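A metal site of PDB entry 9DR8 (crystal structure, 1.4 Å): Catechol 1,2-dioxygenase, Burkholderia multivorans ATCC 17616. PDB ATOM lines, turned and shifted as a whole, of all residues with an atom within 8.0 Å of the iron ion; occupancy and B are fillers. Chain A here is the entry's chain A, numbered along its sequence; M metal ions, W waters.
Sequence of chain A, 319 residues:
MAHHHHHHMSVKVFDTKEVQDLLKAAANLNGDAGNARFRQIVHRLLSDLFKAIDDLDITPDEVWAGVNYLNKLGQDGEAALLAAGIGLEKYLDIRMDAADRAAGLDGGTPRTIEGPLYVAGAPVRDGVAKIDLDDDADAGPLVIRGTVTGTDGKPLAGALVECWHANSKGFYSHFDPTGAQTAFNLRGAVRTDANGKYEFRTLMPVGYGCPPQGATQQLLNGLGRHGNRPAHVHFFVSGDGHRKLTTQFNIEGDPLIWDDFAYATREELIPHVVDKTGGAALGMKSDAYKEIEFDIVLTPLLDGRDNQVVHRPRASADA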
ATOM      1  N   ILE A 113     -24.780 -32.867  21.089  1.00  0.00           N
ATOM      2  CA  ILE A 113     -24.759 -33.238  19.681  1.00  0.00           C
ATOM      3  C   ILE A 113     -23.518 -32.669  19.001  1.00  0.00           C
ATOM      4  O   ILE A 113     -23.050 -31.560  19.298  1.00  0.00           O
ATOM      5  CB  ILE A 113     -26.063 -32.838  18.958  1.00  0.00           C
ATOM      6  CG1 ILE A 113     -26.164 -31.328  18.793  1.00  0.00           C
ATOM      7  CG2 ILE A 113     -27.263 -33.420  19.702  1.00  0.00           C
ATOM      8  CD1 ILE A 113     -27.347 -30.892  17.947  1.00  0.00           C
ATOM      9  N   GLU A 114     -22.993 -33.441  18.052  1.00  0.00           N
ATOM     10  CA  GLU A 114     -21.878 -33.004  17.210  1.00  0.00           C
ATOM     11  C   GLU A 114     -22.284 -31.866  16.274  1.00  0.00           C
ATOM     12  O   GLU A 114     -21.489 -30.956  16.031  1.00  0.00           O
ATOM     13  CB  GLU A 114     -21.407 -34.195  16.387  1.00  0.00           C
ATOM     14  CG  GLU A 114     -20.208 -33.918  15.518  1.00  0.00           C
ATOM     15  CD  GLU A 114     -19.708 -35.161  14.803  1.00  0.00           C
ATOM     16  OE1 GLU A 114     -19.861 -36.278  15.343  1.00  0.00           O
ATOM     17  OE2 GLU A 114     -19.174 -35.024  13.679  1.00  0.00           O
ATOM     18  N   GLY A 115     -23.492 -31.931  15.714  1.00  0.00           N
ATOM     19  CA  GLY A 115     -23.859 -31.073  14.614  1.00  0.00           C
ATOM     20  C   GLY A 115     -23.173 -31.502  13.337  1.00  0.00           C
ATOM     21  O   GLY A 115     -22.339 -32.422  13.336  1.00  0.00           O
ATOM     22  N   PRO A 116     -23.475 -30.823  12.222  1.00  0.00           N
ATOM     23  CA  PRO A 116     -22.996 -31.289  10.909  1.00  0.00           C
ATOM     24  C   PRO A 116     -21.735 -30.607  10.392  1.00  0.00           C
ATOM     25  O   PRO A 116     -21.389 -30.824   9.219  1.00  0.00           O
ATOM     26  CB  PRO A 116     -24.193 -30.951  10.010  1.00  0.00           C
ATOM     27  CG  PRO A 116     -24.789 -29.716  10.612  1.00  0.00           C
ATOM     28  CD  PRO A 116     -24.594 -29.869  12.105  1.00  0.00           C
ATOM     29  N   LEU A 117     -21.017 -29.842  11.209  1.00  0.00           N
ATOM     30  CA  LEU A 117     -19.999 -28.945  10.683  1.00  0.00           C
ATOM     31  C   LEU A 117     -18.580 -29.247  11.133  1.00  0.00           C
ATOM     32  O   LEU A 117     -17.706 -28.394  11.017  1.00  0.00           O
ATOM     33  CB  LEU A 117     -20.362 -27.485  10.957  1.00  0.00           C
ATOM     34  CG  LEU A 117     -21.770 -27.087  10.507  1.00  0.00           C
ATOM     35  CD1 LEU A 117     -21.982 -25.617  10.838  1.00  0.00           C
ATOM     36  CD2 LEU A 117     -22.018 -27.339   9.019  1.00  0.00           C
ATOM     37  N   TYR A 118     -18.299 -30.452  11.620  1.00  0.00           N
ATOM     38  CA  TYR A 118     -16.916 -30.820  11.886  1.00  0.00           C
ATOM     39  C   TYR A 118     -16.129 -30.902  10.588  1.00  0.00           C
ATOM     40  O   TYR A 118     -16.661 -31.325   9.556  1.00  0.00           O
ATOM     41  CB  TYR A 118     -16.845 -32.171  12.596  1.00  0.00           C
ATOM     42  CG  TYR A 118     -15.447 -32.641  12.917  1.00  0.00           C
ATOM     43  CD1 TYR A 118     -14.690 -32.017  13.911  1.00  0.00           C
ATOM     44  CD2 TYR A 118     -14.868 -33.715  12.250  1.00  0.00           C
ATOM     45  CE1 TYR A 118     -13.415 -32.441  14.212  1.00  0.00           C
ATOM     46  CE2 TYR A 118     -13.597 -34.152  12.548  1.00  0.00           C
ATOM     47  CZ  TYR A 118     -12.878 -33.523  13.542  1.00  0.00           C
ATOM     48  OH  TYR A 118     -11.613 -33.966  13.844  1.00  0.00           O
ATOM     49  N   TRP A 164     -14.334 -26.399  17.457  1.00  0.00           N
ATOM     50  CA  TRP A 164     -14.690 -25.658  16.259  1.00  0.00           C
ATOM     51  C   TRP A 164     -15.882 -24.767  16.586  1.00  0.00           C
ATOM     52  O   TRP A 164     -16.739 -25.137  17.397  1.00  0.00           O
ATOM     53  CB  TRP A 164     -14.942 -26.580  15.036  1.00  0.00           C
ATOM     54  CG  TRP A 164     -16.086 -27.582  15.104  1.00  0.00           C
ATOM     55  CD1 TRP A 164     -17.288 -27.490  14.463  1.00  0.00           C
ATOM     56  CD2 TRP A 164     -16.099 -28.832  15.799  1.00  0.00           C
ATOM     57  NE1 TRP A 164     -18.060 -28.606  14.730  1.00  0.00           N
ATOM     58  CE2 TRP A 164     -17.348 -29.437  15.556  1.00  0.00           C
ATOM     59  CE3 TRP A 164     -15.181 -29.495  16.626  1.00  0.00           C
ATOM     60  CZ2 TRP A 164     -17.704 -30.672  16.107  1.00  0.00           C
ATOM     61  CZ3 TRP A 164     -15.540 -30.714  17.175  1.00  0.00           C
ATOM     62  CH2 TRP A 164     -16.778 -31.295  16.915  1.00  0.00           C
ATOM     63  N   HIS A 165     -15.929 -23.587  15.980  1.00  0.00           N
ATOM     64  CA  HIS A 165     -17.009 -22.653  16.257  1.00  0.00           C
ATOM     65  C   HIS A 165     -17.127 -21.615  15.145  1.00  0.00           C
ATOM     66  O   HIS A 165     -16.267 -21.526  14.258  1.00  0.00           O
ATOM     67  CB  HIS A 165     -16.854 -21.982  17.637  1.00  0.00           C
ATOM     68  CG  HIS A 165     -15.702 -21.023  17.731  1.00  0.00           C
ATOM     69  ND1 HIS A 165     -15.783 -19.715  17.301  1.00  0.00           N
ATOM     70  CD2 HIS A 165     -14.469 -21.157  18.281  1.00  0.00           C
ATOM     71  CE1 HIS A 165     -14.637 -19.099  17.546  1.00  0.00           C
ATOM     72  NE2 HIS A 165     -13.817 -19.959  18.128  1.00  0.00           N
ATOM     73  N   ALA A 166     -18.184 -20.815  15.221  1.00  0.00           N
ATOM     74  CA  ALA A 166     -18.557 -19.852  14.204  1.00  0.00           C
ATOM     75  C   ALA A 166     -17.900 -18.492  14.439  1.00  0.00           C
ATOM     76  O   ALA A 166     -17.458 -18.165  15.544  1.00  0.00           O
ATOM     77  CB  ALA A 166     -20.075 -19.655  14.189  1.00  0.00           C
ATOM     78  N   GLY A 170     -21.860 -15.849  12.150  1.00  0.00           N
ATOM     79  CA  GLY A 170     -22.505 -17.128  12.308  1.00  0.00           C
ATOM     80  C   GLY A 170     -22.011 -18.202  11.389  1.00  0.00           C
ATOM     81  O   GLY A 170     -22.660 -19.254  11.291  1.00  0.00           O
ATOM     82  N   TYR A 172     -18.991 -20.878   9.786  1.00  0.00           N
ATOM     83  CA  TYR A 172     -17.831 -21.710  10.064  1.00  0.00           C
ATOM     84  C   TYR A 172     -16.973 -21.804   8.808  1.00  0.00           C
ATOM     85  O   TYR A 172     -17.477 -21.796   7.676  1.00  0.00           O
ATOM     86  CB  TYR A 172     -18.257 -23.125  10.415  1.00  0.00           C
ATOM     87  CG  TYR A 172     -18.971 -23.317  11.731  1.00  0.00           C
ATOM     88  CD1 TYR A 172     -20.272 -22.883  11.917  1.00  0.00           C
ATOM     89  CD2 TYR A 172     -18.369 -24.016  12.766  1.00  0.00           C
ATOM     90  CE1 TYR A 172     -20.941 -23.099  13.116  1.00  0.00           C
ATOM     91  CE2 TYR A 172     -19.009 -24.234  13.961  1.00  0.00           C
ATOM     92  CZ  TYR A 172     -20.298 -23.776  14.129  1.00  0.00           C
ATOM     93  OH  TYR A 172     -20.943 -24.007  15.320  1.00  0.00           O
ATOM     94  N   VAL A 206     -20.758 -16.208  17.614  1.00  0.00           N
ATOM     95  CA  VAL A 206     -22.144 -15.781  17.634  1.00  0.00           C
ATOM     96  C   VAL A 206     -22.977 -16.949  17.115  1.00  0.00           C
ATOM     97  O   VAL A 206     -22.485 -17.796  16.361  1.00  0.00           O
ATOM     98  CB  VAL A 206     -22.340 -14.521  16.754  1.00  0.00           C
ATOM     99  CG1 VAL A 206     -23.803 -14.145  16.623  1.00  0.00           C
ATOM    100  CG2 VAL A 206     -21.552 -13.366  17.327  1.00  0.00           C
ATOM    101  N   GLY A 207     -24.230 -17.001  17.553  1.00  0.00           N
ATOM    102  CA  GLY A 207     -25.150 -18.007  17.086  1.00  0.00           C
ATOM    103  C   GLY A 207     -25.492 -17.781  15.626  1.00  0.00           C
ATOM    104  O   GLY A 207     -25.049 -16.833  14.972  1.00  0.00           O
ATOM    105  N   TYR A 208     -26.304 -18.676  15.089  1.00  0.00           N
ATOM    106  CA  TYR A 208     -26.555 -18.633  13.651  1.00  0.00           C
ATOM    107  C   TYR A 208     -27.861 -19.336  13.359  1.00  0.00           C
ATOM    108  O   TYR A 208     -28.388 -20.077  14.189  1.00  0.00           O
ATOM    109  CB  TYR A 208     -25.423 -19.301  12.880  1.00  0.00           C
ATOM    110  CG  TYR A 208     -25.053 -20.657  13.414  1.00  0.00           C
ATOM    111  CD1 TYR A 208     -24.099 -20.800  14.417  1.00  0.00           C
ATOM    112  CD2 TYR A 208     -25.655 -21.803  12.923  1.00  0.00           C
ATOM    113  CE1 TYR A 208     -23.752 -22.053  14.909  1.00  0.00           C
ATOM    114  CE2 TYR A 208     -25.323 -23.048  13.403  1.00  0.00           C
ATOM    115  CZ  TYR A 208     -24.378 -23.177  14.392  1.00  0.00           C
ATOM    116  OH  TYR A 208     -24.049 -24.427  14.836  1.00  0.00           O
ATOM    117  N   ARG A 229     -29.654 -21.143  16.473  1.00  0.00           N
ATOM    118  CA  ARG A 229     -28.916 -21.714  17.580  1.00  0.00           C
ATOM    119  C   ARG A 229     -28.255 -20.612  18.384  1.00  0.00           C
ATOM    120  O   ARG A 229     -27.792 -19.621  17.806  1.00  0.00           O
ATOM    121  CB  ARG A 229     -27.803 -22.646  17.092  1.00  0.00           C
ATOM    122  CG  ARG A 229     -28.249 -23.667  16.068  1.00  0.00           C
ATOM    123  CD  ARG A 229     -27.301 -24.847  16.000  1.00  0.00           C
ATOM    124  NE  ARG A 229     -27.372 -25.636  17.237  1.00  0.00           N
ATOM    125  CZ  ARG A 229     -26.521 -26.586  17.580  1.00  0.00           C
ATOM    126  NH1 ARG A 229     -25.497 -26.909  16.801  1.00  0.00           N
ATOM    127  NH2 ARG A 229     -26.704 -27.237  18.720  1.00  0.00           N
ATOM    128  N   PRO A 230     -28.200 -20.742  19.698  1.00  0.00           N
ATOM    129  CA  PRO A 230     -27.415 -19.795  20.495  1.00  0.00           C
ATOM    130  C   PRO A 230     -25.931 -20.040  20.285  1.00  0.00           C
ATOM    131  O   PRO A 230     -25.525 -21.093  19.799  1.00  0.00           O
ATOM    132  CB  PRO A 230     -27.829 -20.142  21.932  1.00  0.00           C
ATOM    133  CG  PRO A 230     -28.102 -21.620  21.860  1.00  0.00           C
ATOM    134  CD  PRO A 230     -28.745 -21.842  20.514  1.00  0.00           C
ATOM    135  N   ALA A 231     -25.121 -19.059  20.664  1.00  0.00           N
ATOM    136  CA  ALA A 231     -23.672 -19.176  20.481  1.00  0.00           C
ATOM    137  C   ALA A 231     -23.097 -20.315  21.313  1.00  0.00           C
ATOM    138  O   ALA A 231     -23.462 -20.517  22.471  1.00  0.00           O
ATOM    139  CB  ALA A 231     -23.007 -17.859  20.878  1.00  0.00           C
ATOM    140  N   HIS A 232     -22.150 -21.041  20.721  1.00  0.00           N
ATOM    141  CA  HIS A 232     -21.588 -22.238  21.342  1.00  0.00           C
ATOM    142  C   HIS A 232     -20.237 -22.561  20.704  1.00  0.00           C
ATOM    143  O   HIS A 232     -19.886 -22.035  19.650  1.00  0.00           O
ATOM    144  CB  HIS A 232     -22.526 -23.441  21.166  1.00  0.00           C
ATOM    145  CG  HIS A 232     -22.818 -23.753  19.733  1.00  0.00           C
ATOM    146  ND1 HIS A 232     -23.808 -23.111  19.027  1.00  0.00           N
ATOM    147  CD2 HIS A 232     -22.244 -24.633  18.880  1.00  0.00           C
ATOM    148  CE1 HIS A 232     -23.834 -23.586  17.795  1.00  0.00           C
ATOM    149  NE2 HIS A 232     -22.894 -24.503  17.669  1.00  0.00           N
ATOM    150  N   VAL A 233     -19.498 -23.428  21.392  1.00  0.00           N
ATOM    151  CA  VAL A 233     -18.227 -23.977  20.905  1.00  0.00           C
ATOM    152  C   VAL A 233     -18.320 -25.495  20.999  1.00  0.00           C
ATOM    153  O   VAL A 233     -18.682 -26.041  22.054  1.00  0.00           O
ATOM    154  CB  VAL A 233     -17.030 -23.450  21.720  1.00  0.00           C
ATOM    155  CG1 VAL A 233     -15.728 -24.069  21.194  1.00  0.00           C
ATOM    156  CG2 VAL A 233     -16.978 -21.928  21.666  1.00  0.00           C
ATOM    157  N   HIS A 234     -18.008 -26.181  19.906  1.00  0.00           N
ATOM    158  CA  HIS A 234     -18.019 -27.634  19.841  1.00  0.00           C
ATOM    159  C   HIS A 234     -16.689 -28.229  20.295  1.00  0.00           C
ATOM    160  O   HIS A 234     -15.624 -27.646  20.072  1.00  0.00           O
ATOM    161  CB  HIS A 234     -18.217 -28.090  18.396  1.00  0.00           C
ATOM    162  CG  HIS A 234     -19.522 -27.705  17.794  1.00  0.00           C
ATOM    163  ND1 HIS A 234     -20.640 -28.511  17.873  1.00  0.00           N
ATOM    164  CD2 HIS A 234     -19.886 -26.626  17.071  1.00  0.00           C
ATOM    165  CE1 HIS A 234     -21.640 -27.927  17.231  1.00  0.00           C
ATOM    166  NE2 HIS A 234     -21.209 -26.771  16.743  1.00  0.00           N
ATOM    167  N   GLN A 248     -20.093 -29.752  23.973  1.00  0.00           N
ATOM    168  CA  GLN A 248     -20.024 -28.349  23.607  1.00  0.00           C
ATOM    169  C   GLN A 248     -20.155 -27.531  24.877  1.00  0.00           C
ATOM    170  O   GLN A 248     -20.494 -28.048  25.939  1.00  0.00           O
ATOM    171  CB  GLN A 248     -21.137 -27.959  22.629  1.00  0.00           C
ATOM    172  CG  GLN A 248     -22.429 -27.511  23.241  1.00  0.00           C
ATOM    173  CD  GLN A 248     -23.487 -27.147  22.206  1.00  0.00           C
ATOM    174  OE1 GLN A 248     -24.487 -26.505  22.532  1.00  0.00           O
ATOM    175  NE2 GLN A 248     -23.248 -27.524  20.955  1.00  0.00           N
HETATM  176 FE    FE M   1     -22.354 -25.300  15.753  1.00  0.00          FE
HETATM  177  O   HOH W   1     -22.994 -26.832  14.518  1.00  0.00           O
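N of His 234 is in hydrogen-bond range of O of Trp 164 (3.0 Å). A ring nitrogen (ND1) of His 234 lies within hydrogen-bond range of the backbone carbonyl oxygen (O) of Glu 114, 3.2 Å away. O of Tyr 208 is in hydrogen-bond range of N of Arg 229 (2.8 Å). A ring nitrogen (ND1) of His 232 is in hydrogen-bond range of the backbone carbonyl oxygen of Pro 230.
Merely in contact with the iron ion: Arg 229. Five residues have an atom within 4 Å of the iron ion: Tyr 172, Tyr 208, Arg 229, His 232 and His 234. The nearest printed residue that does not touch the iron ion is Leu 117 (4.9 Å).
The side-chain hydroxyl (OH) of Tyr 172 binds the iron ion (2.0 Å). Water W1 is bound to the iron ion, 2.1 Å away. A ring nitrogen (NE2) of His 234 is bound to the iron ion. The iron ion is bound by the side-chain hydroxyl (OH) of Tyr 208 (2.1 Å). A ring nitrogen (NE2) of His 232 binds the iron ion (2.1 Å). The iron ion has five donor atoms within binding distance.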
